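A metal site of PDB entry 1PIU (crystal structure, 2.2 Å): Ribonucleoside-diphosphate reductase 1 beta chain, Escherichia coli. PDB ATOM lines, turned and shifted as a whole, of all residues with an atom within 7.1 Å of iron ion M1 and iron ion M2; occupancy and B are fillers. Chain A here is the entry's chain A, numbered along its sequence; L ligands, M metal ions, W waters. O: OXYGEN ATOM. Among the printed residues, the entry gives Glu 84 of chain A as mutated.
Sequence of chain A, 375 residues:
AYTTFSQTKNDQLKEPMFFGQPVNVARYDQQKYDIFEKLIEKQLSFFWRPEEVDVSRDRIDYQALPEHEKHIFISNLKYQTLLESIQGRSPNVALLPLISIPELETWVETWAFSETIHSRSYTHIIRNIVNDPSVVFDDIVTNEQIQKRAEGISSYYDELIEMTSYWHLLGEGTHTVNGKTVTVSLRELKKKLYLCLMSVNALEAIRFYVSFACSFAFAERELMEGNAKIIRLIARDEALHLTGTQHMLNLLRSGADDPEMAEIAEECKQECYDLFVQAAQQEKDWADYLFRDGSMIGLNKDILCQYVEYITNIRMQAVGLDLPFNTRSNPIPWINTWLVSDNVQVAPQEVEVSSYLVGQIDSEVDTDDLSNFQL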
ATOM      1  N   GLN A  80     -18.922  34.437 -25.296  1.00  0.00           N
ATOM      2  CA  GLN A  80     -18.640  33.061 -25.695  1.00  0.00           C
ATOM      3  C   GLN A  80     -19.819  32.542 -26.538  1.00  0.00           C
ATOM      4  O   GLN A  80     -19.641  31.894 -27.567  1.00  0.00           O
ATOM      5  CB  GLN A  80     -18.445  32.167 -24.453  1.00  0.00           C
ATOM      6  CG  GLN A  80     -17.266  32.584 -23.559  1.00  0.00           C
ATOM      7  CD  GLN A  80     -17.180  31.792 -22.252  1.00  0.00           C
ATOM      8  OE1 GLN A  80     -18.155  31.710 -21.499  1.00  0.00           O
ATOM      9  NE2 GLN A  80     -16.011  31.212 -21.985  1.00  0.00           N
ATOM     10  N   LEU A  83     -19.782  34.052 -30.165  1.00  0.00           N
ATOM     11  CA  LEU A  83     -18.793  33.381 -31.003  1.00  0.00           C
ATOM     12  C   LEU A  83     -19.168  31.939 -31.337  1.00  0.00           C
ATOM     13  O   LEU A  83     -18.944  31.482 -32.453  1.00  0.00           O
ATOM     14  CB  LEU A  83     -17.418  33.401 -30.345  1.00  0.00           C
ATOM     15  CG  LEU A  83     -16.771  34.761 -30.057  1.00  0.00           C
ATOM     16  CD1 LEU A  83     -15.364  34.552 -29.496  1.00  0.00           C
ATOM     17  CD2 LEU A  83     -16.723  35.606 -31.329  1.00  0.00           C
ATOM     18  N   GLU A  84     -19.730  31.224 -30.362  1.00  0.00           N
ATOM     19  CA  GLU A  84     -20.117  29.835 -30.533  1.00  0.00           C
ATOM     20  C   GLU A  84     -21.234  29.715 -31.584  1.00  0.00           C
ATOM     21  O   GLU A  84     -21.210  28.826 -32.424  1.00  0.00           O
ATOM     22  CB  GLU A  84     -20.594  29.260 -29.194  1.00  0.00           C
ATOM     23  CG  GLU A  84     -20.023  27.905 -28.829  1.00  0.00           C
ATOM     24  CD  GLU A  84     -18.499  27.847 -28.875  1.00  0.00           C
ATOM     25  OE1 GLU A  84     -17.946  27.735 -29.991  1.00  0.00           O
ATOM     26  OE2 GLU A  84     -17.864  27.913 -27.810  1.00  0.00           O
ATOM     27  N   GLN A  87     -19.603  30.139 -34.876  1.00  0.00           N
ATOM     28  CA  GLN A  87     -18.746  28.996 -35.200  1.00  0.00           C
ATOM     29  C   GLN A  87     -19.518  27.717 -35.513  1.00  0.00           C
ATOM     30  O   GLN A  87     -18.983  26.793 -36.123  1.00  0.00           O
ATOM     31  CB  GLN A  87     -17.759  28.745 -34.058  1.00  0.00           C
ATOM     32  CG  GLN A  87     -16.598  29.717 -34.043  1.00  0.00           C
ATOM     33  CD  GLN A  87     -15.898  29.795 -35.384  1.00  0.00           C
ATOM     34  OE1 GLN A  87     -16.294  30.568 -36.269  1.00  0.00           O
ATOM     35  NE2 GLN A  87     -14.861  28.985 -35.561  1.00  0.00           N
ATOM     36  N   TRP A 111     -16.111  19.436 -36.829  1.00  0.00           N
ATOM     37  CA  TRP A 111     -15.713  20.629 -36.086  1.00  0.00           C
ATOM     38  C   TRP A 111     -16.931  21.531 -35.888  1.00  0.00           C
ATOM     39  O   TRP A 111     -17.207  21.993 -34.778  1.00  0.00           O
ATOM     40  CB  TRP A 111     -14.589  21.306 -36.885  1.00  0.00           C
ATOM     41  CG  TRP A 111     -14.230  22.718 -36.534  1.00  0.00           C
ATOM     42  CD1 TRP A 111     -14.386  23.337 -35.327  1.00  0.00           C
ATOM     43  CD2 TRP A 111     -13.590  23.662 -37.401  1.00  0.00           C
ATOM     44  NE1 TRP A 111     -13.874  24.620 -35.392  1.00  0.00           N
ATOM     45  CE2 TRP A 111     -13.381  24.836 -36.645  1.00  0.00           C
ATOM     46  CE3 TRP A 111     -13.179  23.622 -38.738  1.00  0.00           C
ATOM     47  CZ2 TRP A 111     -12.758  25.975 -37.196  1.00  0.00           C
ATOM     48  CZ3 TRP A 111     -12.563  24.751 -39.277  1.00  0.00           C
ATOM     49  CH2 TRP A 111     -12.362  25.916 -38.508  1.00  0.00           C
ATOM     50  N   SER A 114     -19.351  20.063 -33.276  1.00  0.00           N
ATOM     51  CA  SER A 114     -18.911  20.195 -31.887  1.00  0.00           C
ATOM     52  C   SER A 114     -19.194  21.615 -31.382  1.00  0.00           C
ATOM     53  O   SER A 114     -19.351  21.844 -30.188  1.00  0.00           O
ATOM     54  CB  SER A 114     -17.426  19.855 -31.750  1.00  0.00           C
ATOM     55  OG  SER A 114     -16.609  20.861 -32.304  1.00  0.00           O
ATOM     56  N   GLU A 115     -19.258  22.571 -32.308  1.00  0.00           N
ATOM     57  CA  GLU A 115     -19.542  23.956 -31.944  1.00  0.00           C
ATOM     58  C   GLU A 115     -21.001  24.096 -31.480  1.00  0.00           C
ATOM     59  O   GLU A 115     -21.272  24.820 -30.515  1.00  0.00           O
ATOM     60  CB  GLU A 115     -19.268  24.898 -33.123  1.00  0.00           C
ATOM     61  CG  GLU A 115     -17.804  24.898 -33.583  1.00  0.00           C
ATOM     62  CD  GLU A 115     -16.834  25.385 -32.523  1.00  0.00           C
ATOM     63  OE1 GLU A 115     -17.157  25.276 -31.317  1.00  0.00           O
ATOM     64  OE2 GLU A 115     -15.727  25.864 -32.876  1.00  0.00           O
ATOM     65  N   THR A 116     -21.932  23.413 -32.144  1.00  0.00           N
ATOM     66  CA  THR A 116     -23.337  23.508 -31.737  1.00  0.00           C
ATOM     67  C   THR A 116     -23.490  22.893 -30.347  1.00  0.00           C
ATOM     68  O   THR A 116     -24.348  23.311 -29.562  1.00  0.00           O
ATOM     69  CB  THR A 116     -24.300  22.761 -32.714  1.00  0.00           C
ATOM     70  OG1 THR A 116     -23.990  21.366 -32.762  1.00  0.00           O
ATOM     71  CG2 THR A 116     -24.211  23.365 -34.113  1.00  0.00           C
ATOM     72  N   HIS A 118     -21.262  23.104 -28.020  1.00  0.00           N
ATOM     73  CA  HIS A 118     -20.813  24.159 -27.131  1.00  0.00           C
ATOM     74  C   HIS A 118     -21.934  25.190 -26.928  1.00  0.00           C
ATOM     75  O   HIS A 118     -22.176  25.660 -25.806  1.00  0.00           O
ATOM     76  CB  HIS A 118     -19.575  24.853 -27.708  1.00  0.00           C
ATOM     77  CG  HIS A 118     -18.383  23.942 -27.824  1.00  0.00           C
ATOM     78  ND1 HIS A 118     -17.208  24.325 -28.424  1.00  0.00           N
ATOM     79  CD2 HIS A 118     -18.195  22.655 -27.420  1.00  0.00           C
ATOM     80  CE1 HIS A 118     -16.350  23.330 -28.393  1.00  0.00           C
ATOM     81  NE2 HIS A 118     -16.930  22.301 -27.788  1.00  0.00           N
ATOM     82  N   SER A 119     -22.617  25.546 -28.010  1.00  0.00           N
ATOM     83  CA  SER A 119     -23.710  26.498 -27.914  1.00  0.00           C
ATOM     84  C   SER A 119     -24.801  25.918 -27.021  1.00  0.00           C
ATOM     85  O   SER A 119     -25.437  26.642 -26.253  1.00  0.00           O
ATOM     86  CB  SER A 119     -24.285  26.816 -29.297  1.00  0.00           C
ATOM     87  OG  SER A 119     -23.320  27.466 -30.095  1.00  0.00           O
ATOM     88  N   TYR A 122     -23.961  26.260 -23.413  1.00  0.00           N
ATOM     89  CA  TYR A 122     -24.171  27.603 -22.888  1.00  0.00           C
ATOM     90  C   TYR A 122     -25.642  27.862 -22.511  1.00  0.00           C
ATOM     91  O   TYR A 122     -25.917  28.547 -21.531  1.00  0.00           O
ATOM     92  CB  TYR A 122     -23.690  28.654 -23.896  1.00  0.00           C
ATOM     93  CG  TYR A 122     -22.177  28.704 -24.036  1.00  0.00           C
ATOM     94  CD1 TYR A 122     -21.349  28.717 -22.914  1.00  0.00           C
ATOM     95  CD2 TYR A 122     -21.575  28.752 -25.292  1.00  0.00           C
ATOM     96  CE1 TYR A 122     -19.955  28.767 -23.032  1.00  0.00           C
ATOM     97  CE2 TYR A 122     -20.184  28.809 -25.430  1.00  0.00           C
ATOM     98  CZ  TYR A 122     -19.380  28.815 -24.298  1.00  0.00           C
ATOM     99  OH  TYR A 122     -18.013  28.877 -24.431  1.00  0.00           O
ATOM    100  N   VAL A 200     -10.008  32.787 -38.317  1.00  0.00           N
ATOM    101  CA  VAL A 200     -10.621  31.752 -37.494  1.00  0.00           C
ATOM    102  C   VAL A 200      -9.582  31.242 -36.501  1.00  0.00           C
ATOM    103  O   VAL A 200      -9.892  30.902 -35.366  1.00  0.00           O
ATOM    104  CB  VAL A 200     -11.179  30.554 -38.334  1.00  0.00           C
ATOM    105  CG1 VAL A 200     -10.086  29.942 -39.168  1.00  0.00           C
ATOM    106  CG2 VAL A 200     -11.768  29.493 -37.418  1.00  0.00           C
ATOM    107  N   GLU A 204     -10.329  31.266 -32.436  1.00  0.00           N
ATOM    108  CA  GLU A 204     -10.288  30.126 -31.535  1.00  0.00           C
ATOM    109  C   GLU A 204      -9.036  30.030 -30.668  1.00  0.00           C
ATOM    110  O   GLU A 204      -9.093  29.587 -29.526  1.00  0.00           O
ATOM    111  CB  GLU A 204     -10.432  28.841 -32.334  1.00  0.00           C
ATOM    112  CG  GLU A 204     -11.736  28.762 -33.099  1.00  0.00           C
ATOM    113  CD  GLU A 204     -11.932  27.425 -33.760  1.00  0.00           C
ATOM    114  OE1 GLU A 204     -11.035  27.011 -34.526  1.00  0.00           O
ATOM    115  OE2 GLU A 204     -12.981  26.793 -33.521  1.00  0.00           O
ATOM    116  N   PHE A 208     -11.122  32.978 -27.692  1.00  0.00           N
ATOM    117  CA  PHE A 208     -11.732  32.027 -26.780  1.00  0.00           C
ATOM    118  C   PHE A 208     -10.893  31.696 -25.556  1.00  0.00           C
ATOM    119  O   PHE A 208     -11.447  31.426 -24.488  1.00  0.00           O
ATOM    120  CB  PHE A 208     -12.097  30.729 -27.525  1.00  0.00           C
ATOM    121  CG  PHE A 208     -13.522  30.704 -28.024  1.00  0.00           C
ATOM    122  CD1 PHE A 208     -14.579  30.657 -27.118  1.00  0.00           C
ATOM    123  CD2 PHE A 208     -13.801  30.736 -29.383  1.00  0.00           C
ATOM    124  CE1 PHE A 208     -15.904  30.643 -27.562  1.00  0.00           C
ATOM    125  CE2 PHE A 208     -15.125  30.724 -29.840  1.00  0.00           C
ATOM    126  CZ  PHE A 208     -16.171  30.679 -28.926  1.00  0.00           C
ATOM    127  N   PHE A 212     -11.730  31.855 -21.656  1.00  0.00           N
ATOM    128  CA  PHE A 212     -11.555  30.712 -20.763  1.00  0.00           C
ATOM    129  C   PHE A 212     -10.940  31.214 -19.452  1.00  0.00           C
ATOM    130  O   PHE A 212     -11.350  30.796 -18.366  1.00  0.00           O
ATOM    131  CB  PHE A 212     -10.623  29.659 -21.368  1.00  0.00           C
ATOM    132  CG  PHE A 212     -11.151  29.008 -22.623  1.00  0.00           C
ATOM    133  CD1 PHE A 212     -12.509  28.988 -22.907  1.00  0.00           C
ATOM    134  CD2 PHE A 212     -10.274  28.389 -23.517  1.00  0.00           C
ATOM    135  CE1 PHE A 212     -12.994  28.356 -24.047  1.00  0.00           C
ATOM    136  CE2 PHE A 212     -10.746  27.761 -24.663  1.00  0.00           C
ATOM    137  CZ  PHE A 212     -12.111  27.745 -24.940  1.00  0.00           C
ATOM    138  N   ILE A 234     -14.992  22.237 -23.290  1.00  0.00           N
ATOM    139  CA  ILE A 234     -14.969  23.073 -24.480  1.00  0.00           C
ATOM    140  C   ILE A 234     -13.527  23.381 -24.890  1.00  0.00           C
ATOM    141  O   ILE A 234     -13.165  23.226 -26.053  1.00  0.00           O
ATOM    142  CB  ILE A 234     -15.735  24.394 -24.239  1.00  0.00           C
ATOM    143  CG1 ILE A 234     -17.233  24.093 -24.200  1.00  0.00           C
ATOM    144  CG2 ILE A 234     -15.395  25.417 -25.315  1.00  0.00           C
ATOM    145  CD1 ILE A 234     -18.088  25.327 -24.008  1.00  0.00           C
ATOM    146  N   ASP A 237     -11.916  20.740 -26.739  1.00  0.00           N
ATOM    147  CA  ASP A 237     -12.308  20.667 -28.158  1.00  0.00           C
ATOM    148  C   ASP A 237     -11.595  21.746 -28.958  1.00  0.00           C
ATOM    149  O   ASP A 237     -11.089  21.498 -30.046  1.00  0.00           O
ATOM    150  CB  ASP A 237     -13.822  20.882 -28.329  1.00  0.00           C
ATOM    151  CG  ASP A 237     -14.649  19.741 -27.785  1.00  0.00           C
ATOM    152  OD1 ASP A 237     -14.144  18.594 -27.717  1.00  0.00           O
ATOM    153  OD2 ASP A 237     -15.831  19.995 -27.450  1.00  0.00           O
ATOM    154  N   GLU A 238     -11.557  22.956 -28.388  1.00  0.00           N
ATOM    155  CA  GLU A 238     -10.929  24.110 -29.029  1.00  0.00           C
ATOM    156  C   GLU A 238      -9.471  23.858 -29.393  1.00  0.00           C
ATOM    157  O   GLU A 238      -8.984  24.346 -30.419  1.00  0.00           O
ATOM    158  CB  GLU A 238     -11.035  25.325 -28.115  1.00  0.00           C
ATOM    159  CG  GLU A 238     -10.856  26.645 -28.856  1.00  0.00           C
ATOM    160  CD  GLU A 238     -12.022  26.958 -29.786  1.00  0.00           C
ATOM    161  OE1 GLU A 238     -12.859  27.812 -29.411  1.00  0.00           O
ATOM    162  OE2 GLU A 238     -12.114  26.348 -30.876  1.00  0.00           O
ATOM    163  N   ALA A 239      -8.766  23.094 -28.568  1.00  0.00           N
ATOM    164  CA  ALA A 239      -7.367  22.780 -28.838  1.00  0.00           C
ATOM    165  C   ALA A 239      -7.264  22.006 -30.156  1.00  0.00           C
ATOM    166  O   ALA A 239      -6.305  22.192 -30.904  1.00  0.00           O
ATOM    167  CB  ALA A 239      -6.781  21.939 -27.690  1.00  0.00           C
ATOM    168  N   HIS A 241      -9.526  22.221 -32.634  1.00  0.00           N
ATOM    169  CA  HIS A 241      -9.942  23.171 -33.656  1.00  0.00           C
ATOM    170  C   HIS A 241      -8.791  24.049 -34.148  1.00  0.00           C
ATOM    171  O   HIS A 241      -8.578  24.181 -35.348  1.00  0.00           O
ATOM    172  CB  HIS A 241     -11.065  24.068 -33.126  1.00  0.00           C
ATOM    173  CG  HIS A 241     -12.283  23.319 -32.676  1.00  0.00           C
ATOM    174  ND1 HIS A 241     -13.386  23.950 -32.134  1.00  0.00           N
ATOM    175  CD2 HIS A 241     -12.584  22.002 -32.708  1.00  0.00           C
ATOM    176  CE1 HIS A 241     -14.315  23.052 -31.851  1.00  0.00           C
ATOM    177  NE2 HIS A 241     -13.850  21.866 -32.186  1.00  0.00           N
ATOM    178  N   LEU A 242      -8.078  24.668 -33.213  1.00  0.00           N
ATOM    179  CA  LEU A 242      -6.964  25.535 -33.574  1.00  0.00           C
ATOM    180  C   LEU A 242      -5.808  24.724 -34.147  1.00  0.00           C
ATOM    181  O   LEU A 242      -5.011  25.235 -34.937  1.00  0.00           O
ATOM    182  CB  LEU A 242      -6.500  26.366 -32.368  1.00  0.00           C
ATOM    183  CG  LEU A 242      -5.792  25.719 -31.183  1.00  0.00           C
ATOM    184  CD1 LEU A 242      -4.308  25.543 -31.506  1.00  0.00           C
ATOM    185  CD2 LEU A 242      -5.942  26.602 -29.950  1.00  0.00           C
HETATM  186  O     O L   1     -14.572  25.551 -29.739  1.00  0.00           O
HETATM  187 FE    FE M   1     -13.875  25.989 -31.774  1.00  0.00          FE
HETATM  188 FE    FE M   2     -16.399  26.244 -29.604  1.00  0.00          FE
HETATM  189  O   HOH W   1     -14.937  27.168 -27.928  1.00  0.00           O
HETATM  190  O   HOH W   2     -14.741  27.848 -31.154  1.00  0.00           O
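The nearest printed residue that does not touch iron ion M2 is His 241 (4.4 Å).
The indole nitrogen (NE1) of Trp 111 lies close to the side-chain carboxylate (OE2) of Glu 115 (3.4 Å). The side-chain carboxylate (OE2) of Glu 204 sits close to the indole nitrogen (NE1) of Trp 111 (3.0 Å). The indole nitrogen (NE1) of Trp 111 lies close to a ring nitrogen (ND1) of His 241 (3.4 Å). NE2 of His 241 sits at hydrogen-bond distance from OG of Ser 114 (2.9 Å). The backbone carbonyl oxygen (O) of Glu 84 sits close to the side-chain hydroxyl (OG) of Ser 119 (3.4 Å). The backbone carbonyl oxygen (O) of Ser 114 sits close to a ring nitrogen (NE2) of His 118, 3.4 Å away. A ring nitrogen (NE2) of His 118 is in hydrogen-bond range of the side-chain carboxylate (OD2) of Asp 237, at 2.6 Å. The backbone carbonyl oxygen (O) of Trp 111 is in hydrogen-bond range of the side-chain hydroxyl (OG) of Ser 114 (2.8 Å).
Iron ion M1 is bound by OE2 of Glu 238, OE2 of Glu 204, ND1 of His 241, water W2, OE2 of Glu 115 and O of the ligand. Iron ion M1 has six donor atoms within binding distance.
Iron ion M2 is bound by an oxygen (O) of the ligand (2.0 Å), the side-chain carboxylate (OE1) of Glu 115 (2.1 Å), the side-chain carboxylate (OE1) of Glu 84 (2.2 Å), a ring nitrogen (ND1) of His 118 (2.4 Å) and water W1 (2.4 Å). Slightly farther from iron ion M2 lies water W2 (2.8 Å).
Residues that only touch iron ion M1: Trp 111. Within 4 Å of iron ion M1: Trp 111, Glu 115, Glu 204, Glu 238 and His 241. The nearest printed residue that does not touch iron ion M1 is Glu 84 (4.8 Å).
Water W1 lies within hydrogen-bond range of OE1 of Glu 238 (2.6 Å) and OE2 of Glu 84 (3.0 Å).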
